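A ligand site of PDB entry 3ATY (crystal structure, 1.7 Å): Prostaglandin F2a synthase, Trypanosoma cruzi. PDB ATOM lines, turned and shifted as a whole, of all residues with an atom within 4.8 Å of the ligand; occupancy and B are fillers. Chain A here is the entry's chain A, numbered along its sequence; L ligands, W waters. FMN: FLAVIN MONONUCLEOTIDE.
The side-chain amide nitrogen (ND2) of Asn 313 lies within hydrogen-bond range of an oxygen (O3') of the ligand (2.6 Å).
The backbone NH of Thr 28 is in hydrogen-bond range of a nitrogen (N5) of the ligand (2.6 Å).
O4 of the ligand sits at hydrogen-bond distance from OG1 of Thr 28, 2.6 Å away.
N3 of the ligand lies within hydrogen-bond range of OE1 of Gln 103 (2.8 Å).
The backbone NH (N) of Arg 315 is in hydrogen-bond range of an oxygen (O1P) of the ligand.
The guanidinium group (NH2) of Arg 249 lies within hydrogen-bond range of an oxygen (O2) of the ligand (2.8 Å).
N of Ala 337 lies within hydrogen-bond range of O3P of the ligand, 2.8 Å away.
N of Gly 336 lies within hydrogen-bond range of O2P of the ligand (2.9 Å).
An oxygen (O2') of the ligand lies within hydrogen-bond range of the backbone carbonyl oxygen (O) of Pro 26, at 3.0 Å.
An oxygen (O2) of the ligand is in hydrogen-bond range of a ring nitrogen (NE2) of His 195 (3.1 Å).
The backbone NH of Ala 61 is in hydrogen-bond range of an oxygen (O4) of the ligand (3.2 Å).
The side-chain amide nitrogen of Asn 198 sits at hydrogen-bond distance from an oxygen (O2) of the ligand (3.3 Å).
The guanidinium group of Arg 249 sits close to the side-chain amide nitrogen of Asn 313 (3.2 Å).
The side-chain amide oxygen of Asn 313 lies close to the backbone carbonyl oxygen of Ala 334, at 2.8 Å.
OE1 of Gln 103 sits close to N of Ala 61, 3.4 Å away.
The backbone carbonyl oxygen (O) of Met 290 sits at hydrogen-bond distance from the guanidinium group (NH1) of Arg 315, at 3.5 Å.
N of Ala 25 lies within hydrogen-bond range of O of Phe 335 (3.0 Å).
The guanidinium group of Arg 29 is in hydrogen-bond range of the backbone carbonyl oxygen of Tyr 363 (2.9 Å).
Merely in contact with the ligand: Ala 25 (3.5 Å), Leu 27 (3.3 Å), Leu 286 (3.7 Å), Leu 314 (3.5 Å), Phe 335 (3.7 Å), Tyr 363 (3.6 Å) and Tyr 364 (3.1 Å).
Water W2 lies within hydrogen-bond range of an oxygen (O2P) of the ligand (2.7 Å), the backbone carbonyl oxygen of Ala 334 (2.9 Å), the backbone NH of Leu 314 (3.0 Å), the side-chain amide oxygen of Asn 313 (3.4 Å) and the backbone NH of Tyr 316 (3.4 Å).
Water W5 lies within hydrogen-bond range of O2P of the ligand (2.8 Å), N of Ala 337 (3.4 Å) and N of Gly 336 (3.5 Å).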
ATOM      1  N   ALA A  25       0.474  -8.965  -6.533  1.00  0.00           N
ATOM      2  CA  ALA A  25       0.716  -9.634  -7.805  1.00  0.00           C
ATOM      3  C   ALA A  25       2.193  -9.562  -8.188  1.00  0.00           C
ATOM      4  O   ALA A  25       2.910  -8.657  -7.756  1.00  0.00           O
ATOM      5  CB  ALA A  25      -0.133  -8.996  -8.891  1.00  0.00           C
ATOM      6  N   PRO A  26       2.660 -10.512  -9.007  1.00  0.00           N
ATOM      7  CA  PRO A  26       4.059 -10.515  -9.442  1.00  0.00           C
ATOM      8  C   PRO A  26       4.279  -9.279 -10.325  1.00  0.00           C
ATOM      9  O   PRO A  26       3.531  -9.058 -11.274  1.00  0.00           O
ATOM     10  CB  PRO A  26       4.183 -11.830 -10.206  1.00  0.00           C
ATOM     11  CG  PRO A  26       2.801 -12.055 -10.744  1.00  0.00           C
ATOM     12  CD  PRO A  26       1.928 -11.667  -9.571  1.00  0.00           C
ATOM     13  N   LEU A  27       5.288  -8.489 -10.016  1.00  0.00           N
ATOM     14  CA  LEU A  27       5.546  -7.278 -10.786  1.00  0.00           C
ATOM     15  C   LEU A  27       7.016  -7.099 -11.156  1.00  0.00           C
ATOM     16  O   LEU A  27       7.850  -6.798 -10.305  1.00  0.00           O
ATOM     17  CB  LEU A  27       5.076  -6.055  -9.990  1.00  0.00           C
ATOM     18  CG  LEU A  27       3.586  -6.024  -9.615  1.00  0.00           C
ATOM     19  CD1 LEU A  27       3.390  -5.251  -8.322  1.00  0.00           C
ATOM     20  CD2 LEU A  27       2.770  -5.410 -10.755  1.00  0.00           C
ATOM     21  N   THR A  28       7.309  -7.298 -12.438  1.00  0.00           N
ATOM     22  CA  THR A  28       8.661  -7.126 -12.969  1.00  0.00           C
ATOM     23  C   THR A  28       9.073  -5.662 -12.792  1.00  0.00           C
ATOM     24  O   THR A  28       8.415  -4.769 -13.322  1.00  0.00           O
ATOM     25  CB  THR A  28       8.695  -7.473 -14.469  1.00  0.00           C
ATOM     26  OG1 THR A  28       8.534  -8.886 -14.630  1.00  0.00           O
ATOM     27  CG2 THR A  28      10.000  -7.036 -15.099  1.00  0.00           C
ATOM     28  N   ARG A  29      10.149  -5.427 -12.046  1.00  0.00           N
ATOM     29  CA  ARG A  29      10.621  -4.062 -11.827  1.00  0.00           C
ATOM     30  C   ARG A  29      12.040  -3.836 -12.357  1.00  0.00           C
ATOM     31  O   ARG A  29      12.578  -2.731 -12.270  1.00  0.00           O
ATOM     32  CB  ARG A  29      10.544  -3.702 -10.333  1.00  0.00           C
ATOM     33  CG  ARG A  29       9.172  -3.942  -9.690  1.00  0.00           C
ATOM     34  CD  ARG A  29       8.040  -3.241 -10.449  1.00  0.00           C
ATOM     35  NE  ARG A  29       8.246  -1.799 -10.556  1.00  0.00           N
ATOM     36  CZ  ARG A  29       8.061  -0.935  -9.549  1.00  0.00           C
ATOM     37  NH1 ARG A  29       8.283   0.358  -9.740  1.00  0.00           N
ATOM     38  NH2 ARG A  29       7.644  -1.355  -8.370  1.00  0.00           N
ATOM     39  N   GLU A  60       8.188 -11.024  -8.385  1.00  0.00           N
ATOM     40  CA  GLU A  60       8.276 -10.833  -9.830  1.00  0.00           C
ATOM     41  C   GLU A  60       8.826 -12.016 -10.618  1.00  0.00           C
ATOM     42  O   GLU A  60       9.597 -12.812 -10.095  1.00  0.00           O
ATOM     43  CB  GLU A  60       9.154  -9.609 -10.122  1.00  0.00           C
ATOM     44  CG  GLU A  60      10.568  -9.768  -9.601  1.00  0.00           C
ATOM     45  CD  GLU A  60      11.211  -8.442  -9.293  1.00  0.00           C
ATOM     46  OE1 GLU A  60      11.540  -7.708 -10.247  1.00  0.00           O
ATOM     47  OE2 GLU A  60      11.381  -8.138  -8.100  1.00  0.00           O
ATOM     48  N   ALA A  61       8.435 -12.081 -11.883  1.00  0.00           N
ATOM     49  CA  ALA A  61       8.874 -13.137 -12.793  1.00  0.00           C
ATOM     50  C   ALA A  61      10.392 -13.282 -12.709  1.00  0.00           C
ATOM     51  O   ALA A  61      11.120 -12.316 -12.915  1.00  0.00           O
ATOM     52  CB  ALA A  61       8.456 -12.809 -14.210  1.00  0.00           C
ATOM     53  N   GLN A 103       7.698 -16.262  -8.589  1.00  0.00           N
ATOM     54  CA  GLN A 103       7.121 -16.612  -9.891  1.00  0.00           C
ATOM     55  C   GLN A 103       8.263 -17.040 -10.792  1.00  0.00           C
ATOM     56  O   GLN A 103       9.279 -16.339 -10.901  1.00  0.00           O
ATOM     57  CB  GLN A 103       6.386 -15.424 -10.519  1.00  0.00           C
ATOM     58  CG  GLN A 103       5.615 -15.840 -11.774  1.00  0.00           C
ATOM     59  CD  GLN A 103       4.986 -14.681 -12.519  1.00  0.00           C
ATOM     60  OE1 GLN A 103       5.676 -13.742 -12.907  1.00  0.00           O
ATOM     61  NE2 GLN A 103       3.681 -14.752 -12.734  1.00  0.00           N
ATOM     62  N   HIS A 195       4.645 -19.438 -14.134  1.00  0.00           N
ATOM     63  CA  HIS A 195       4.144 -18.393 -15.028  1.00  0.00           C
ATOM     64  C   HIS A 195       3.587 -18.972 -16.315  1.00  0.00           C
ATOM     65  O   HIS A 195       4.326 -19.188 -17.274  1.00  0.00           O
ATOM     66  CB  HIS A 195       5.249 -17.386 -15.364  1.00  0.00           C
ATOM     67  CG  HIS A 195       4.725 -16.076 -15.876  1.00  0.00           C
ATOM     68  ND1 HIS A 195       3.529 -15.969 -16.549  1.00  0.00           N
ATOM     69  CD2 HIS A 195       5.219 -14.827 -15.779  1.00  0.00           C
ATOM     70  CE1 HIS A 195       3.303 -14.702 -16.849  1.00  0.00           C
ATOM     71  NE2 HIS A 195       4.317 -13.983 -16.392  1.00  0.00           N
ATOM     72  N   ASN A 198       0.432 -14.335 -19.827  1.00  0.00           N
ATOM     73  CA  ASN A 198       0.950 -13.193 -20.568  1.00  0.00           C
ATOM     74  C   ASN A 198       1.863 -13.391 -21.775  1.00  0.00           C
ATOM     75  O   ASN A 198       2.795 -12.619 -21.992  1.00  0.00           O
ATOM     76  CB  ASN A 198       1.615 -12.230 -19.569  1.00  0.00           C
ATOM     77  CG  ASN A 198       0.728 -11.949 -18.371  1.00  0.00           C
ATOM     78  OD1 ASN A 198      -0.503 -11.941 -18.490  1.00  0.00           O
ATOM     79  ND2 ASN A 198       1.341 -11.699 -17.214  1.00  0.00           N
ATOM     80  N   ARG A 249      -0.253 -19.467 -12.612  1.00  0.00           N
ATOM     81  CA  ARG A 249      -0.917 -18.287 -13.131  1.00  0.00           C
ATOM     82  C   ARG A 249      -1.236 -18.411 -14.619  1.00  0.00           C
ATOM     83  O   ARG A 249      -0.409 -18.900 -15.400  1.00  0.00           O
ATOM     84  CB  ARG A 249      -0.078 -17.019 -12.910  1.00  0.00           C
ATOM     85  CG  ARG A 249      -0.906 -15.746 -13.102  1.00  0.00           C
ATOM     86  CD  ARG A 249      -0.127 -14.448 -12.882  1.00  0.00           C
ATOM     87  NE  ARG A 249      -1.012 -13.427 -12.335  1.00  0.00           N
ATOM     88  CZ  ARG A 249      -0.813 -12.108 -12.433  1.00  0.00           C
ATOM     89  NH1 ARG A 249      -1.685 -11.270 -11.886  1.00  0.00           N
ATOM     90  NH2 ARG A 249       0.225 -11.625 -13.095  1.00  0.00           N
ATOM     91  N   LEU A 286      -5.768 -13.816 -14.631  1.00  0.00           N
ATOM     92  CA  LEU A 286      -6.174 -12.470 -15.012  1.00  0.00           C
ATOM     93  C   LEU A 286      -7.566 -12.734 -15.549  1.00  0.00           C
ATOM     94  O   LEU A 286      -7.766 -13.638 -16.375  1.00  0.00           O
ATOM     95  CB  LEU A 286      -5.273 -11.903 -16.121  1.00  0.00           C
ATOM     96  CG  LEU A 286      -4.079 -11.054 -15.678  1.00  0.00           C
ATOM     97  CD1 LEU A 286      -3.024 -11.930 -15.019  1.00  0.00           C
ATOM     98  CD2 LEU A 286      -3.483 -10.355 -16.904  1.00  0.00           C
ATOM     99  N   MET A 290      -5.348  -7.080 -20.833  1.00  0.00           N
ATOM    100  CA  MET A 290      -4.532  -5.917 -20.536  1.00  0.00           C
ATOM    101  C   MET A 290      -4.687  -4.873 -21.639  1.00  0.00           C
ATOM    102  O   MET A 290      -4.545  -3.678 -21.395  1.00  0.00           O
ATOM    103  CB  MET A 290      -3.048  -6.319 -20.444  1.00  0.00           C
ATOM    104  CG  MET A 290      -2.716  -7.310 -19.349  1.00  0.00           C
ATOM    105  SD  MET A 290      -2.545  -6.534 -17.743  1.00  0.00           S
ATOM    106  CE  MET A 290      -0.795  -6.145 -17.755  1.00  0.00           C
ATOM    107  N   ASN A 313      -7.388 -11.451 -10.631  1.00  0.00           N
ATOM    108  CA  ASN A 313      -6.616 -10.238 -10.826  1.00  0.00           C
ATOM    109  C   ASN A 313      -7.036  -9.453 -12.058  1.00  0.00           C
ATOM    110  O   ASN A 313      -7.604 -10.012 -12.993  1.00  0.00           O
ATOM    111  CB  ASN A 313      -5.134 -10.585 -10.974  1.00  0.00           C
ATOM    112  CG  ASN A 313      -4.311  -9.411 -11.462  1.00  0.00           C
ATOM    113  OD1 ASN A 313      -3.864  -8.565 -10.672  1.00  0.00           O
ATOM    114  ND2 ASN A 313      -4.125  -9.324 -12.772  1.00  0.00           N
ATOM    115  N   LEU A 314      -6.758  -8.149 -12.014  1.00  0.00           N
ATOM    116  CA  LEU A 314      -6.984  -7.173 -13.085  1.00  0.00           C
ATOM    117  C   LEU A 314      -8.065  -6.125 -12.834  1.00  0.00           C
ATOM    118  O   LEU A 314      -9.262  -6.399 -12.862  1.00  0.00           O
ATOM    119  CB  LEU A 314      -7.245  -7.851 -14.440  1.00  0.00           C
ATOM    120  CG  LEU A 314      -7.268  -6.902 -15.636  1.00  0.00           C
ATOM    121  CD1 LEU A 314      -5.922  -6.181 -15.768  1.00  0.00           C
ATOM    122  CD2 LEU A 314      -7.566  -7.681 -16.911  1.00  0.00           C
ATOM    123  N   ARG A 315      -7.592  -4.900 -12.593  1.00  0.00           N
ATOM    124  CA  ARG A 315      -8.457  -3.748 -12.362  1.00  0.00           C
ATOM    125  C   ARG A 315      -9.468  -3.885 -11.231  1.00  0.00           C
ATOM    126  O   ARG A 315     -10.619  -3.488 -11.369  1.00  0.00           O
ATOM    127  CB  ARG A 315      -9.154  -3.378 -13.677  1.00  0.00           C
ATOM    128  CG  ARG A 315      -8.177  -3.057 -14.799  1.00  0.00           C
ATOM    129  CD  ARG A 315      -8.881  -2.559 -16.060  1.00  0.00           C
ATOM    130  NE  ARG A 315      -7.926  -2.113 -17.071  1.00  0.00           N
ATOM    131  CZ  ARG A 315      -7.360  -2.905 -17.983  1.00  0.00           C
ATOM    132  NH1 ARG A 315      -6.497  -2.402 -18.850  1.00  0.00           N
ATOM    133  NH2 ARG A 315      -7.681  -4.186 -18.044  1.00  0.00           N
ATOM    134  N   TYR A 316      -9.015  -4.456 -10.116  1.00  0.00           N
ATOM    135  CA  TYR A 316      -9.842  -4.605  -8.929  1.00  0.00           C
ATOM    136  C   TYR A 316      -9.521  -3.479  -7.968  1.00  0.00           C
ATOM    137  O   TYR A 316      -8.420  -2.939  -7.968  1.00  0.00           O
ATOM    138  CB  TYR A 316      -9.543  -5.904  -8.189  1.00  0.00           C
ATOM    139  CG  TYR A 316     -10.241  -7.131  -8.695  1.00  0.00           C
ATOM    140  CD1 TYR A 316      -9.639  -7.950  -9.643  1.00  0.00           C
ATOM    141  CD2 TYR A 316     -11.494  -7.494  -8.200  1.00  0.00           C
ATOM    142  CE1 TYR A 316     -10.266  -9.116 -10.081  1.00  0.00           C
ATOM    143  CE2 TYR A 316     -12.124  -8.647  -8.635  1.00  0.00           C
ATOM    144  CZ  TYR A 316     -11.509  -9.459  -9.567  1.00  0.00           C
ATOM    145  OH  TYR A 316     -12.126 -10.604  -9.986  1.00  0.00           O
ATOM    146  N   ALA A 334      -5.371 -10.433  -6.258  1.00  0.00           N
ATOM    147  CA  ALA A 334      -4.005  -9.931  -6.356  1.00  0.00           C
ATOM    148  C   ALA A 334      -4.070  -8.554  -6.993  1.00  0.00           C
ATOM    149  O   ALA A 334      -4.749  -8.354  -8.002  1.00  0.00           O
ATOM    150  CB  ALA A 334      -3.156 -10.865  -7.191  1.00  0.00           C
ATOM    151  N   PHE A 335      -3.358  -7.598  -6.395  1.00  0.00           N
ATOM    152  CA  PHE A 335      -3.305  -6.235  -6.880  1.00  0.00           C
ATOM    153  C   PHE A 335      -1.906  -5.949  -7.401  1.00  0.00           C
ATOM    154  O   PHE A 335      -0.911  -6.286  -6.752  1.00  0.00           O
ATOM    155  CB  PHE A 335      -3.636  -5.262  -5.757  1.00  0.00           C
ATOM    156  CG  PHE A 335      -5.021  -5.410  -5.202  1.00  0.00           C
ATOM    157  CD1 PHE A 335      -6.089  -4.728  -5.774  1.00  0.00           C
ATOM    158  CD2 PHE A 335      -5.263  -6.249  -4.123  1.00  0.00           C
ATOM    159  CE1 PHE A 335      -7.382  -4.872  -5.273  1.00  0.00           C
ATOM    160  CE2 PHE A 335      -6.545  -6.401  -3.602  1.00  0.00           C
ATOM    161  CZ  PHE A 335      -7.606  -5.716  -4.181  1.00  0.00           C
ATOM    162  N   GLY A 336      -1.826  -5.342  -8.584  1.00  0.00           N
ATOM    163  CA  GLY A 336      -0.530  -5.024  -9.161  1.00  0.00           C
ATOM    164  C   GLY A 336      -0.189  -3.550  -8.974  1.00  0.00           C
ATOM    165  O   GLY A 336       0.615  -3.199  -8.114  1.00  0.00           O
ATOM    166  N   ALA A 337      -0.818  -2.693  -9.773  1.00  0.00           N
ATOM    167  CA  ALA A 337      -0.564  -1.264  -9.707  1.00  0.00           C
ATOM    168  C   ALA A 337      -0.689  -0.679  -8.301  1.00  0.00           C
ATOM    169  O   ALA A 337       0.121   0.143  -7.891  1.00  0.00           O
ATOM    170  CB  ALA A 337      -1.505  -0.530 -10.661  1.00  0.00           C
ATOM    171  N   ILE A 340       2.355  -1.384  -6.228  1.00  0.00           N
ATOM    172  CA  ILE A 340       3.528  -0.630  -6.660  1.00  0.00           C
ATOM    173  C   ILE A 340       3.504   0.715  -5.947  1.00  0.00           C
ATOM    174  O   ILE A 340       4.506   1.160  -5.380  1.00  0.00           O
ATOM    175  CB  ILE A 340       3.509  -0.364  -8.189  1.00  0.00           C
ATOM    176  CG1 ILE A 340       3.742  -1.660  -8.955  1.00  0.00           C
ATOM    177  CG2 ILE A 340       4.570   0.676  -8.552  1.00  0.00           C
ATOM    178  CD1 ILE A 340       3.680  -1.490 -10.468  1.00  0.00           C
ATOM    179  N   TYR A 363       7.561   2.868 -13.726  1.00  0.00           N
ATOM    180  CA  TYR A 363       7.581   1.480 -13.284  1.00  0.00           C
ATOM    181  C   TYR A 363       8.912   0.742 -13.484  1.00  0.00           C
ATOM    182  O   TYR A 363       9.252  -0.156 -12.722  1.00  0.00           O
ATOM    183  CB  TYR A 363       6.495   0.665 -13.989  1.00  0.00           C
ATOM    184  CG  TYR A 363       5.065   0.967 -13.590  1.00  0.00           C
ATOM    185  CD1 TYR A 363       4.771   1.644 -12.407  1.00  0.00           C
ATOM    186  CD2 TYR A 363       4.001   0.508 -14.355  1.00  0.00           C
ATOM    187  CE1 TYR A 363       3.451   1.876 -12.008  1.00  0.00           C
ATOM    188  CE2 TYR A 363       2.681   0.720 -13.965  1.00  0.00           C
ATOM    189  CZ  TYR A 363       2.408   1.397 -12.793  1.00  0.00           C
ATOM    190  OH  TYR A 363       1.114   1.592 -12.399  1.00  0.00           O
ATOM    191  N   TYR A 364       9.660   1.135 -14.515  1.00  0.00           N
ATOM    192  CA  TYR A 364      10.914   0.451 -14.838  1.00  0.00           C
ATOM    193  C   TYR A 364      12.151   1.334 -14.883  1.00  0.00           C
ATOM    194  O   TYR A 364      13.010   1.149 -15.753  1.00  0.00           O
ATOM    195  CB  TYR A 364      10.769  -0.233 -16.200  1.00  0.00           C
ATOM    196  CG  TYR A 364       9.504  -1.044 -16.400  1.00  0.00           C
ATOM    197  CD1 TYR A 364       9.434  -2.383 -16.009  1.00  0.00           C
ATOM    198  CD2 TYR A 364       8.379  -0.486 -17.012  1.00  0.00           C
ATOM    199  CE1 TYR A 364       8.275  -3.141 -16.227  1.00  0.00           C
ATOM    200  CE2 TYR A 364       7.237  -1.231 -17.238  1.00  0.00           C
ATOM    201  CZ  TYR A 364       7.183  -2.557 -16.854  1.00  0.00           C
ATOM    202  OH  TYR A 364       6.048  -3.308 -17.076  1.00  0.00           O
HETATM  203  N1  FMN L   1       2.489 -10.303 -14.334  1.00  0.00           N
HETATM  204  C2  FMN L   1       3.183 -11.475 -14.209  1.00  0.00           C
HETATM  205  O2  FMN L   1       2.602 -12.586 -14.252  1.00  0.00           O
HETATM  206  N3  FMN L   1       4.575 -11.440 -14.002  1.00  0.00           N
HETATM  207  C4  FMN L   1       5.309 -10.242 -13.945  1.00  0.00           C
HETATM  208  O4  FMN L   1       6.564 -10.312 -13.728  1.00  0.00           O
HETATM  209  C4A FMN L   1       4.611  -9.008 -14.088  1.00  0.00           C
HETATM  210  N5  FMN L   1       5.262  -7.817 -14.027  1.00  0.00           N
HETATM  211  C5A FMN L   1       4.551  -6.629 -14.145  1.00  0.00           C
HETATM  212  C6  FMN L   1       5.206  -5.351 -14.070  1.00  0.00           C
HETATM  213  C7  FMN L   1       4.528  -4.116 -14.163  1.00  0.00           C
HETATM  214  C7M FMN L   1       5.296  -2.830 -14.062  1.00  0.00           C
HETATM  215  C8  FMN L   1       3.077  -4.149 -14.340  1.00  0.00           C
HETATM  216  C8M FMN L   1       2.233  -2.877 -14.445  1.00  0.00           C
HETATM  217  C9  FMN L   1       2.409  -5.364 -14.413  1.00  0.00           C
HETATM  218  C9A FMN L   1       3.106  -6.639 -14.320  1.00  0.00           C
HETATM  219  N10 FMN L   1       2.449  -7.914 -14.382  1.00  0.00           N
HETATM  220  C10 FMN L   1       3.166  -9.129 -14.270  1.00  0.00           C
HETATM  221  C1' FMN L   1       0.978  -7.977 -14.519  1.00  0.00           C
HETATM  222  C2' FMN L   1       0.443  -7.801 -13.071  1.00  0.00           C
HETATM  223  O2' FMN L   1       0.753  -8.968 -12.273  1.00  0.00           O
HETATM  224  C3' FMN L   1      -1.060  -7.615 -12.989  1.00  0.00           C
HETATM  225  O3' FMN L   1      -1.731  -8.800 -13.523  1.00  0.00           O
HETATM  226  C4' FMN L   1      -1.562  -6.364 -13.773  1.00  0.00           C
HETATM  227  O4' FMN L   1      -0.858  -5.213 -13.222  1.00  0.00           O
HETATM  228  C5' FMN L   1      -3.045  -6.129 -13.692  1.00  0.00           C
HETATM  229  O5' FMN L   1      -3.424  -6.041 -12.311  1.00  0.00           O
HETATM  230  P   FMN L   1      -3.808  -4.527 -11.648  1.00  0.00           P
HETATM  231  O1P FMN L   1      -4.971  -3.987 -12.453  1.00  0.00           O
HETATM  232  O2P FMN L   1      -4.139  -4.885 -10.224  1.00  0.00           O
HETATM  233  O3P FMN L   1      -2.559  -3.650 -11.786  1.00  0.00           O
HETATM  234  O   HOH W   1      -5.873  -1.360 -11.962  1.00  0.00           O
HETATM  235  O   HOH W   2      -6.278  -6.439  -9.592  1.00  0.00           O
HETATM  236  O   HOH W   3      -4.381  -2.706 -14.884  1.00  0.00           O
HETATM  237  O   HOH W   4      -1.827  -2.045 -14.015  1.00  0.00           O
HETATM  238  O   HOH W   5      -4.011  -2.643  -8.484  1.00  0.00           O
